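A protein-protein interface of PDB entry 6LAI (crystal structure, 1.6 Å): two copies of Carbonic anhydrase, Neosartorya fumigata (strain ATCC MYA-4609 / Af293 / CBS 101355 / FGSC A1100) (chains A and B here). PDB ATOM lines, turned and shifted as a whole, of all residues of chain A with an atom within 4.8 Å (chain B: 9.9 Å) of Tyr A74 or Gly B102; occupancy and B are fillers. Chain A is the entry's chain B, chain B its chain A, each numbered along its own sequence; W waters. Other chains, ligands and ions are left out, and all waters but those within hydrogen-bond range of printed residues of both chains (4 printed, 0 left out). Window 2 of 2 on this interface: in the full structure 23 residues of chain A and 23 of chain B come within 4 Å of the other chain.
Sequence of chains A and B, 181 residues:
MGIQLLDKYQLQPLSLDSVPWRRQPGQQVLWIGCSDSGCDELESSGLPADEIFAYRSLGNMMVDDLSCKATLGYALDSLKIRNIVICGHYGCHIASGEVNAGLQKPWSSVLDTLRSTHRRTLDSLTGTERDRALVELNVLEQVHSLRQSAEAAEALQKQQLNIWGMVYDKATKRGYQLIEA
Of the 24 printed residues of chain B, 8 touch a printed residue of chain A. Hydrophobic or aromatic side chains of chain B that line the printed part of chain A: Leu B58, Ile B94 and Trp B107. Hydrophobic or aromatic side chains of chain A that line the printed part of chain B: Phe A53, Ala A70 and Tyr A74. Among the printed residues, 12 pairs touch across the chains.
Water W1 lies within hydrogen-bond range of the backbone carbonyl oxygen (O) of Gly B102 (2.6 Å), the side-chain carboxylate (OD2) of Asp A77 (2.8 Å) and the side-chain amide nitrogen (NE2) of Gln B104 (3.1 Å). Water W3 lies within hydrogen-bond range of OH of Tyr A74 and OD2 of Asp B36. Water W4 lies within hydrogen-bond range of the backbone carbonyl oxygen of Gly B102 (2.7 Å), the backbone carbonyl oxygen of Ala A70 (2.9 Å) and the backbone NH of Gln B104 (2.9 Å). Water W2 lies within hydrogen-bond range of the backbone NH of Leu B58 and the side-chain hydroxyl of Thr A71.
The side-chain amide oxygen of Asn B100 sits at hydrogen-bond distance from the backbone NH of Gly B102, at 3.0 Å. The backbone carbonyl oxygen (O) of Ser B57 lies within hydrogen-bond range of the backbone NH (N) of Ser B35 (3.0 Å). N of Ile B94 lies close to SG of Cys B92, at 3.6 Å. OD2 of Asp B36 sits at hydrogen-bond distance from N of His B93. The backbone carbonyl oxygen (O) of Tyr A74 is in hydrogen-bond range of the backbone NH (N) of Leu A79 (3.1 Å). OD2 of Asp B36 sits at hydrogen-bond distance from N of Ile B94, at 3.5 Å.
No position is printed for both chains. Of the 12 pairs that touch across the chains among the printed residues, none has its exchanged pair printed and touching as well.
Among the printed residues, pairs that only touch across the chains: Phe A53 with Ser B35 (3.5 Å), Phe A53 with Asp B36 (3.9 Å), Phe A53 with Leu B58 (3.9 Å), Ala A70 with Leu B58 (3.9 Å), Ala A70 with Gln B104 (3.6 Å), Ala A70 with Trp B107 (3.3 Å), Thr A71 with Leu B58 (3.9 Å), Gly A73 with Gln B104 (3.9 Å), Tyr A74 with Ile B94 (3.6 Å), Tyr A74 with Asn B100 (3.8 Å), Tyr A74 with Gly B102 (3.7 Å) and Ser A78 with Asn B100 (3.5 Å).
Of chain B, only Ile B94, Asn B100 and Gly B102 come within 4 Å of Tyr A74. Gly B102 touches one residue of chain A. Of chain B, only Gln B104 (3.9 Å) comes within 4 Å of Gly A73. No residue of chain B comes within 4 Å of Ala A75. Ser A78 touches just one residue of chain B: Asn B100 (3.5 Å). Of the printed residues of chain A, Gln B104 touches Ala A70 (3.6 Å) and Gly A73 (3.9 Å). Of the printed residues of chain A, Trp B107 touches Ala A70 (3.3 Å). Of the printed residues of chain A, Asp B36 touches Phe A53 (3.9 Å). Leu A79 touches none of the printed residues of chain B. Leu B103 touches none of the printed residues of chain A.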
ATOM      1  N   PHE A  53      -8.205  31.672 -11.443  1.00  0.00           N
ATOM      2  CA  PHE A  53      -8.528  31.768 -12.883  1.00  0.00           C
ATOM      3  C   PHE A  53      -9.981  32.219 -12.914  1.00  0.00           C
ATOM      4  O   PHE A  53     -10.860  31.426 -12.606  1.00  0.00           O
ATOM      5  CB  PHE A  53      -8.318  30.426 -13.583  1.00  0.00           C
ATOM      6  CG  PHE A  53      -8.534  30.435 -15.058  1.00  0.00           C
ATOM      7  CD1 PHE A  53      -7.597  30.997 -15.929  1.00  0.00           C
ATOM      8  CD2 PHE A  53      -9.730  29.955 -15.588  1.00  0.00           C
ATOM      9  CE1 PHE A  53      -7.811  30.953 -17.293  1.00  0.00           C
ATOM     10  CE2 PHE A  53      -9.932  29.901 -16.955  1.00  0.00           C
ATOM     11  CZ  PHE A  53      -8.980  30.423 -17.806  1.00  0.00           C
ATOM     12  N   ALA A  70     -16.338  26.844 -23.552  1.00  0.00           N
ATOM     13  CA  ALA A  70     -14.906  27.030 -23.828  1.00  0.00           C
ATOM     14  C   ALA A  70     -14.174  27.316 -22.526  1.00  0.00           C
ATOM     15  O   ALA A  70     -13.037  26.871 -22.340  1.00  0.00           O
ATOM     16  CB  ALA A  70     -14.706  28.137 -24.802  1.00  0.00           C
ATOM     17  N   THR A  71     -14.783  28.126 -21.641  1.00  0.00           N
ATOM     18  CA  THR A  71     -14.115  28.532 -20.399  1.00  0.00           C
ATOM     19  C   THR A  71     -13.991  27.292 -19.510  1.00  0.00           C
ATOM     20  O   THR A  71     -12.937  27.051 -18.959  1.00  0.00           O
ATOM     21  CB  THR A  71     -14.849  29.700 -19.726  1.00  0.00           C
ATOM     22  OG1 THR A  71     -14.852  30.769 -20.660  1.00  0.00           O
ATOM     23  CG2 THR A  71     -14.213  30.144 -18.424  1.00  0.00           C
ATOM     24  N   LEU A  72     -15.112  26.580 -19.357  1.00  0.00           N
ATOM     25  CA  LEU A  72     -15.078  25.356 -18.542  1.00  0.00           C
ATOM     26  C   LEU A  72     -14.094  24.354 -19.151  1.00  0.00           C
ATOM     27  O   LEU A  72     -13.321  23.759 -18.400  1.00  0.00           O
ATOM     28  CB  LEU A  72     -16.502  24.819 -18.461  1.00  0.00           C
ATOM     29  CG  LEU A  72     -16.684  23.570 -17.621  1.00  0.00           C
ATOM     30  CD1 LEU A  72     -16.251  23.822 -16.190  1.00  0.00           C
ATOM     31  CD2 LEU A  72     -18.140  23.118 -17.716  1.00  0.00           C
ATOM     32  N   GLY A  73     -14.162  24.140 -20.468  1.00  0.00           N
ATOM     33  CA  GLY A  73     -13.281  23.190 -21.166  1.00  0.00           C
ATOM     34  C   GLY A  73     -11.824  23.524 -20.967  1.00  0.00           C
ATOM     35  O   GLY A  73     -11.038  22.664 -20.674  1.00  0.00           O
ATOM     36  N   TYR A  74     -11.434  24.798 -21.134  1.00  0.00           N
ATOM     37  CA  TYR A  74     -10.048  25.227 -20.960  1.00  0.00           C
ATOM     38  C   TYR A  74      -9.615  24.944 -19.524  1.00  0.00           C
ATOM     39  O   TYR A  74      -8.545  24.412 -19.248  1.00  0.00           O
ATOM     40  CB  TYR A  74      -9.905  26.719 -21.295  1.00  0.00           C
ATOM     41  CG  TYR A  74      -8.498  27.230 -21.178  1.00  0.00           C
ATOM     42  CD1 TYR A  74      -7.561  26.989 -22.170  1.00  0.00           C
ATOM     43  CD2 TYR A  74      -8.055  27.898 -20.047  1.00  0.00           C
ATOM     44  CE1 TYR A  74      -6.273  27.454 -22.034  1.00  0.00           C
ATOM     45  CE2 TYR A  74      -6.771  28.373 -19.908  1.00  0.00           C
ATOM     46  CZ  TYR A  74      -5.859  28.156 -20.917  1.00  0.00           C
ATOM     47  OH  TYR A  74      -4.559  28.579 -20.728  1.00  0.00           O
ATOM     48  N   ALA A  75     -10.461  25.304 -18.555  1.00  0.00           N
ATOM     49  CA  ALA A  75     -10.157  25.120 -17.139  1.00  0.00           C
ATOM     50  C   ALA A  75      -9.936  23.623 -16.816  1.00  0.00           C
ATOM     51  O   ALA A  75      -8.940  23.335 -16.146  1.00  0.00           O
ATOM     52  CB  ALA A  75     -11.263  25.728 -16.306  1.00  0.00           C
ATOM     53  N   LEU A  76     -10.830  22.756 -17.280  1.00  0.00           N
ATOM     54  CA  LEU A  76     -10.734  21.289 -17.019  1.00  0.00           C
ATOM     55  C   LEU A  76      -9.582  20.678 -17.826  1.00  0.00           C
ATOM     56  O   LEU A  76      -8.810  19.872 -17.241  1.00  0.00           O
ATOM     57  CB  LEU A  76     -12.068  20.628 -17.354  1.00  0.00           C
ATOM     58  CG  LEU A  76     -13.247  21.018 -16.465  1.00  0.00           C
ATOM     59  CD1 LEU A  76     -14.522  20.346 -16.930  1.00  0.00           C
ATOM     60  CD2 LEU A  76     -12.988  20.732 -14.986  1.00  0.00           C
ATOM     61  N   ASP A  77      -9.484  20.992 -19.110  1.00  0.00           N
ATOM     62  CA  ASP A  77      -8.593  20.255 -20.059  1.00  0.00           C
ATOM     63  C   ASP A  77      -7.173  20.816 -20.026  1.00  0.00           C
ATOM     64  O   ASP A  77      -6.211  20.002 -19.980  1.00  0.00           O
ATOM     65  CB  ASP A  77      -9.104  20.286 -21.497  1.00  0.00           C
ATOM     66  CG  ASP A  77     -10.459  19.658 -21.716  1.00  0.00           C
ATOM     67  OD1 ASP A  77     -10.882  18.847 -20.868  1.00  0.00           O
ATOM     68  OD2 ASP A  77     -11.091  19.999 -22.742  1.00  0.00           O
ATOM     69  N   SER A  78      -7.003  22.133 -20.091  1.00  0.00           N
ATOM     70  CA  SER A  78      -5.668  22.769 -20.121  1.00  0.00           C
ATOM     71  C   SER A  78      -5.119  22.987 -18.718  1.00  0.00           C
ATOM     72  O   SER A  78      -3.947  22.723 -18.504  1.00  0.00           O
ATOM     73  CB  SER A  78      -5.695  24.063 -20.889  1.00  0.00           C
ATOM     74  OG  SER A  78      -4.412  24.672 -20.854  1.00  0.00           O
ATOM     75  N   LEU A  79      -5.901  23.545 -17.795  1.00  0.00           N
ATOM     76  CA  LEU A  79      -5.388  23.905 -16.462  1.00  0.00           C
ATOM     77  C   LEU A  79      -5.582  22.758 -15.454  1.00  0.00           C
ATOM     78  O   LEU A  79      -5.053  22.919 -14.372  1.00  0.00           O
ATOM     79  CB  LEU A  79      -6.088  25.164 -15.955  1.00  0.00           C
ATOM     80  CG  LEU A  79      -5.997  26.360 -16.905  1.00  0.00           C
ATOM     81  CD1 LEU A  79      -6.601  27.608 -16.269  1.00  0.00           C
ATOM     82  CD2 LEU A  79      -4.552  26.626 -17.309  1.00  0.00           C
ATOM     83  N   CYS B  34      -8.492  39.489 -19.034  1.00  0.00           N
ATOM     84  CA  CYS B  34      -8.250  38.034 -19.191  1.00  0.00           C
ATOM     85  C   CYS B  34      -8.371  37.256 -17.882  1.00  0.00           C
ATOM     86  O   CYS B  34      -7.877  37.677 -16.838  1.00  0.00           O
ATOM     87  CB  CYS B  34      -6.889  37.809 -19.829  1.00  0.00           C
ATOM     88  SG  CYS B  34      -6.496  36.078 -20.202  1.00  0.00           S
ATOM     89  N   SER B  35      -8.971  36.076 -18.021  1.00  0.00           N
ATOM     90  CA  SER B  35      -9.136  35.096 -16.940  1.00  0.00           C
ATOM     91  C   SER B  35      -7.830  34.654 -16.302  1.00  0.00           C
ATOM     92  O   SER B  35      -7.887  34.420 -15.085  1.00  0.00           O
ATOM     93  CB  SER B  35      -9.904  33.881 -17.441  1.00  0.00           C
ATOM     94  OG  SER B  35     -11.161  34.294 -17.920  1.00  0.00           O
ATOM     95  N   ASP B  36      -6.684  34.688 -16.994  1.00  0.00           N
ATOM     96  CA  ASP B  36      -5.402  34.325 -16.309  1.00  0.00           C
ATOM     97  C   ASP B  36      -4.593  35.567 -15.930  1.00  0.00           C
ATOM     98  O   ASP B  36      -3.431  35.439 -15.505  1.00  0.00           O
ATOM     99  CB  ASP B  36      -4.588  33.294 -17.090  1.00  0.00           C
ATOM    100  CG  ASP B  36      -3.975  33.731 -18.392  1.00  0.00           C
ATOM    101  OD1 ASP B  36      -3.872  34.927 -18.593  1.00  0.00           O
ATOM    102  OD2 ASP B  36      -3.678  32.854 -19.208  1.00  0.00           O
ATOM    103  N   SER B  37      -5.187  36.754 -16.046  1.00  0.00           N
ATOM    104  CA  SER B  37      -4.680  37.956 -15.369  1.00  0.00           C
ATOM    105  C   SER B  37      -5.311  37.991 -13.991  1.00  0.00           C
ATOM    106  O   SER B  37      -5.529  36.900 -13.381  1.00  0.00           O
ATOM    107  CB  SER B  37      -4.958  39.204 -16.194  1.00  0.00           C
ATOM    108  OG  SER B  37      -4.291  40.304 -15.614  1.00  0.00           O
ATOM    109  N   SER B  57     -12.538  37.193 -19.389  1.00  0.00           N
ATOM    110  CA  SER B  57     -12.787  36.131 -20.397  1.00  0.00           C
ATOM    111  C   SER B  57     -11.487  35.526 -20.902  1.00  0.00           C
ATOM    112  O   SER B  57     -10.379  36.062 -20.631  1.00  0.00           O
ATOM    113  CB  SER B  57     -13.505  36.750 -21.588  1.00  0.00           C
ATOM    114  OG  SER B  57     -12.649  37.716 -22.221  1.00  0.00           O
ATOM    115  N   LEU B  58     -11.578  34.435 -21.626  1.00  0.00           N
ATOM    116  CA  LEU B  58     -10.366  33.838 -22.250  1.00  0.00           C
ATOM    117  C   LEU B  58      -9.669  34.857 -23.153  1.00  0.00           C
ATOM    118  O   LEU B  58     -10.264  35.301 -24.140  1.00  0.00           O
ATOM    119  CB  LEU B  58     -10.790  32.627 -23.081  1.00  0.00           C
ATOM    120  CG  LEU B  58     -11.432  31.494 -22.310  1.00  0.00           C
ATOM    121  CD1 LEU B  58     -11.923  30.437 -23.288  1.00  0.00           C
ATOM    122  CD2 LEU B  58     -10.491  30.877 -21.331  1.00  0.00           C
ATOM    123  N   GLY B  59      -8.418  35.158 -22.855  1.00  0.00           N
ATOM    124  CA  GLY B  59      -7.563  36.033 -23.689  1.00  0.00           C
ATOM    125  C   GLY B  59      -8.107  37.441 -23.841  1.00  0.00           C
ATOM    126  O   GLY B  59      -7.722  38.096 -24.834  1.00  0.00           O
ATOM    127  N   HIS B  89      -2.366  41.473 -21.096  1.00  0.00           N
ATOM    128  CA  HIS B  89      -1.345  41.488 -20.020  1.00  0.00           C
ATOM    129  C   HIS B  89      -0.158  40.634 -20.460  1.00  0.00           C
ATOM    130  O   HIS B  89      -0.343  39.518 -20.926  1.00  0.00           O
ATOM    131  CB  HIS B  89      -1.917  41.027 -18.678  1.00  0.00           C
ATOM    132  CG  HIS B  89      -2.441  39.631 -18.678  1.00  0.00           C
ATOM    133  ND1 HIS B  89      -1.881  38.650 -17.877  1.00  0.00           N
ATOM    134  CD2 HIS B  89      -3.346  39.009 -19.478  1.00  0.00           C
ATOM    135  CE1 HIS B  89      -2.523  37.509 -18.145  1.00  0.00           C
ATOM    136  NE2 HIS B  89      -3.358  37.663 -19.171  1.00  0.00           N
ATOM    137  N   GLY B  91       2.747  38.097 -20.274  1.00  0.00           N
ATOM    138  CA  GLY B  91       2.814  36.821 -19.553  1.00  0.00           C
ATOM    139  C   GLY B  91       1.548  36.014 -19.673  1.00  0.00           C
ATOM    140  O   GLY B  91       1.507  34.872 -19.138  1.00  0.00           O
ATOM    141  N   CYS B  92       0.554  36.528 -20.394  1.00  0.00           N
ATOM    142  CA  CYS B  92      -0.688  35.761 -20.699  1.00  0.00           C
ATOM    143  C   CYS B  92      -0.375  34.354 -21.193  1.00  0.00           C
ATOM    144  O   CYS B  92       0.489  34.198 -22.063  1.00  0.00           O
ATOM    145  CB  CYS B  92      -1.481  36.522 -21.750  1.00  0.00           C
ATOM    146  SG  CYS B  92      -3.142  35.875 -22.078  1.00  0.00           S
ATOM    147  N   HIS B  93      -1.039  33.323 -20.681  1.00  0.00           N
ATOM    148  CA  HIS B  93      -0.820  31.945 -21.167  1.00  0.00           C
ATOM    149  C   HIS B  93      -1.722  31.606 -22.339  1.00  0.00           C
ATOM    150  O   HIS B  93      -1.458  30.643 -23.072  1.00  0.00           O
ATOM    151  CB  HIS B  93      -0.999  30.932 -20.033  1.00  0.00           C
ATOM    152  CG  HIS B  93      -0.056  31.177 -18.906  1.00  0.00           C
ATOM    153  ND1 HIS B  93       1.301  30.976 -19.017  1.00  0.00           N
ATOM    154  CD2 HIS B  93      -0.283  31.578 -17.638  1.00  0.00           C
ATOM    155  CE1 HIS B  93       1.878  31.246 -17.863  1.00  0.00           C
ATOM    156  NE2 HIS B  93       0.931  31.614 -17.004  1.00  0.00           N
ATOM    157  N   ILE B  94      -2.795  32.351 -22.531  1.00  0.00           N
ATOM    158  CA  ILE B  94      -3.740  32.106 -23.645  1.00  0.00           C
ATOM    159  C   ILE B  94      -3.208  32.752 -24.908  1.00  0.00           C
ATOM    160  O   ILE B  94      -3.112  32.033 -25.976  1.00  0.00           O
ATOM    161  CB  ILE B  94      -5.135  32.615 -23.221  1.00  0.00           C
ATOM    162  CG1 ILE B  94      -5.645  31.761 -22.050  1.00  0.00           C
ATOM    163  CG2 ILE B  94      -6.096  32.593 -24.410  1.00  0.00           C
ATOM    164  CD1 ILE B  94      -6.864  32.257 -21.311  1.00  0.00           C
ATOM    165  N   ALA B  95      -2.928  34.062 -24.876  1.00  0.00           N
ATOM    166  CA  ALA B  95      -2.363  34.766 -26.050  1.00  0.00           C
ATOM    167  C   ALA B  95      -0.846  34.538 -26.013  1.00  0.00           C
ATOM    168  O   ALA B  95      -0.122  35.471 -25.690  1.00  0.00           O
ATOM    169  CB  ALA B  95      -2.729  36.222 -26.047  1.00  0.00           C
ATOM    170  N   SER B  96      -0.397  33.315 -26.279  1.00  0.00           N
ATOM    171  CA  SER B  96       1.034  32.953 -26.218  1.00  0.00           C
ATOM    172  C   SER B  96       1.320  31.801 -27.165  1.00  0.00           C
ATOM    173  O   SER B  96       0.379  31.086 -27.561  1.00  0.00           O
ATOM    174  CB  SER B  96       1.546  32.673 -24.810  1.00  0.00           C
ATOM    175  OG  SER B  96       1.284  31.362 -24.376  1.00  0.00           O
ATOM    176  N   VAL B  99       0.318  27.165 -30.221  1.00  0.00           N
ATOM    177  CA  VAL B  99      -0.888  26.284 -30.162  1.00  0.00           C
ATOM    178  C   VAL B  99      -1.268  26.062 -28.693  1.00  0.00           C
ATOM    179  O   VAL B  99      -0.369  26.220 -27.838  1.00  0.00           O
ATOM    180  CB  VAL B  99      -0.649  24.981 -30.970  1.00  0.00           C
ATOM    181  CG1 VAL B  99       0.823  24.740 -31.287  1.00  0.00           C
ATOM    182  CG2 VAL B  99      -1.270  23.730 -30.347  1.00  0.00           C
ATOM    183  N   ASN B 100      -2.549  25.783 -28.419  1.00  0.00           N
ATOM    184  CA  ASN B 100      -3.033  25.195 -27.134  1.00  0.00           C
ATOM    185  C   ASN B 100      -4.262  24.318 -27.387  1.00  0.00           C
ATOM    186  O   ASN B 100      -5.327  24.868 -27.725  1.00  0.00           O
ATOM    187  CB  ASN B 100      -3.434  26.230 -26.079  1.00  0.00           C
ATOM    188  CG  ASN B 100      -3.675  25.632 -24.701  1.00  0.00           C
ATOM    189  OD1 ASN B 100      -4.365  24.620 -24.527  1.00  0.00           O
ATOM    190  ND2 ASN B 100      -3.103  26.260 -23.691  1.00  0.00           N
ATOM    191  N   ALA B 101      -4.141  23.011 -27.154  1.00  0.00           N
ATOM    192  CA  ALA B 101      -5.163  22.001 -27.522  1.00  0.00           C
ATOM    193  C   ALA B 101      -6.490  22.268 -26.796  1.00  0.00           C
ATOM    194  O   ALA B 101      -7.553  21.972 -27.389  1.00  0.00           O
ATOM    195  CB  ALA B 101      -4.652  20.608 -27.218  1.00  0.00           C
ATOM    196  N   GLY B 102      -6.437  22.761 -25.555  1.00  0.00           N
ATOM    197  CA  GLY B 102      -7.625  22.913 -24.686  1.00  0.00           C
ATOM    198  C   GLY B 102      -8.399  24.197 -24.983  1.00  0.00           C
ATOM    199  O   GLY B 102      -9.555  24.335 -24.495  1.00  0.00           O
ATOM    200  N   LEU B 103      -7.812  25.093 -25.778  1.00  0.00           N
ATOM    201  CA  LEU B 103      -8.469  26.360 -26.226  1.00  0.00           C
ATOM    202  C   LEU B 103      -9.290  26.113 -27.502  1.00  0.00           C
ATOM    203  O   LEU B 103      -8.740  25.702 -28.525  1.00  0.00           O
ATOM    204  CB  LEU B 103      -7.407  27.442 -26.434  1.00  0.00           C
ATOM    205  CG  LEU B 103      -7.979  28.836 -26.703  1.00  0.00           C
ATOM    206  CD1 LEU B 103      -8.680  29.421 -25.485  1.00  0.00           C
ATOM    207  CD2 LEU B 103      -6.913  29.790 -27.148  1.00  0.00           C
ATOM    208  N   GLN B 104     -10.604  26.305 -27.416  1.00  0.00           N
ATOM    209  CA  GLN B 104     -11.574  25.986 -28.493  1.00  0.00           C
ATOM    210  C   GLN B 104     -11.693  27.163 -29.466  1.00  0.00           C
ATOM    211  O   GLN B 104     -11.194  28.238 -29.170  1.00  0.00           O
ATOM    212  CB  GLN B 104     -12.929  25.662 -27.873  1.00  0.00           C
ATOM    213  CG  GLN B 104     -12.858  24.397 -27.017  1.00  0.00           C
ATOM    214  CD  GLN B 104     -14.071  24.208 -26.138  1.00  0.00           C
ATOM    215  OE1 GLN B 104     -15.170  24.605 -26.508  1.00  0.00           O
ATOM    216  NE2 GLN B 104     -13.898  23.461 -25.049  1.00  0.00           N
ATOM    217  N   LYS B 105     -12.311  26.937 -30.620  1.00  0.00           N
ATOM    218  CA  LYS B 105     -12.720  28.005 -31.551  1.00  0.00           C
ATOM    219  C   LYS B 105     -13.920  28.723 -30.944  1.00  0.00           C
ATOM    220  O   LYS B 105     -14.712  28.099 -30.219  1.00  0.00           O
ATOM    221  CB  LYS B 105     -13.083  27.393 -32.904  1.00  0.00           C
ATOM    222  CG  LYS B 105     -11.929  26.661 -33.562  1.00  0.00           C
ATOM    223  CD  LYS B 105     -12.285  25.836 -34.771  1.00  0.00           C
ATOM    224  CE  LYS B 105     -11.198  24.806 -35.027  1.00  0.00           C
ATOM    225  NZ  LYS B 105     -11.178  24.315 -36.427  1.00  0.00           N
ATOM    226  N   TRP B 107     -11.771  31.257 -30.191  1.00  0.00           N
ATOM    227  CA  TRP B 107     -10.584  31.837 -29.513  1.00  0.00           C
ATOM    228  C   TRP B 107      -9.335  31.357 -30.239  1.00  0.00           C
ATOM    229  O   TRP B 107      -8.436  32.144 -30.508  1.00  0.00           O
ATOM    230  CB  TRP B 107     -10.557  31.514 -28.005  1.00  0.00           C
ATOM    231  CG  TRP B 107     -11.732  32.084 -27.289  1.00  0.00           C
ATOM    232  CD1 TRP B 107     -11.754  33.270 -26.608  1.00  0.00           C
ATOM    233  CD2 TRP B 107     -13.061  31.552 -27.200  1.00  0.00           C
ATOM    234  NE1 TRP B 107     -13.005  33.526 -26.139  1.00  0.00           N
ATOM    235  CE2 TRP B 107     -13.826  32.477 -26.464  1.00  0.00           C
ATOM    236  CE3 TRP B 107     -13.675  30.362 -27.628  1.00  0.00           C
ATOM    237  CZ2 TRP B 107     -15.182  32.296 -26.204  1.00  0.00           C
ATOM    238  CZ3 TRP B 107     -15.002  30.175 -27.346  1.00  0.00           C
ATOM    239  CH2 TRP B 107     -15.747  31.129 -26.648  1.00  0.00           C
ATOM    240  N   SER B 108      -9.267  30.060 -30.544  1.00  0.00           N
ATOM    241  CA  SER B 108      -8.047  29.498 -31.170  1.00  0.00           C
ATOM    242  C   SER B 108      -7.918  30.047 -32.587  1.00  0.00           C
ATOM    243  O   SER B 108      -6.771  30.305 -32.964  1.00  0.00           O
ATOM    244  CB  SER B 108      -8.049  28.011 -31.169  1.00  0.00           C
ATOM    245  OG  SER B 108      -9.185  27.523 -31.870  1.00  0.00           O
ATOM    246  N   LEU B 111      -6.356  33.627 -32.594  1.00  0.00           N
ATOM    247  CA  LEU B 111      -4.894  33.620 -32.390  1.00  0.00           C
ATOM    248  C   LEU B 111      -4.195  33.061 -33.629  1.00  0.00           C
ATOM    249  O   LEU B 111      -3.178  33.552 -33.976  1.00  0.00           O
ATOM    250  CB  LEU B 111      -4.551  32.824 -31.128  1.00  0.00           C
ATOM    251  CG  LEU B 111      -5.063  33.432 -29.825  1.00  0.00           C
ATOM    252  CD1 LEU B 111      -4.889  32.466 -28.682  1.00  0.00           C
ATOM    253  CD2 LEU B 111      -4.389  34.751 -29.513  1.00  0.00           C
HETATM  254  O   HOH W   1     -11.104  22.302 -24.252  1.00  0.00           O
HETATM  255  O   HOH W   2     -14.337  33.437 -21.817  1.00  0.00           O
HETATM  256  O   HOH W   3      -4.328  30.262 -18.725  1.00  0.00           O
HETATM  257  O   HOH W   4     -11.553  26.101 -24.673  1.00  0.00           O
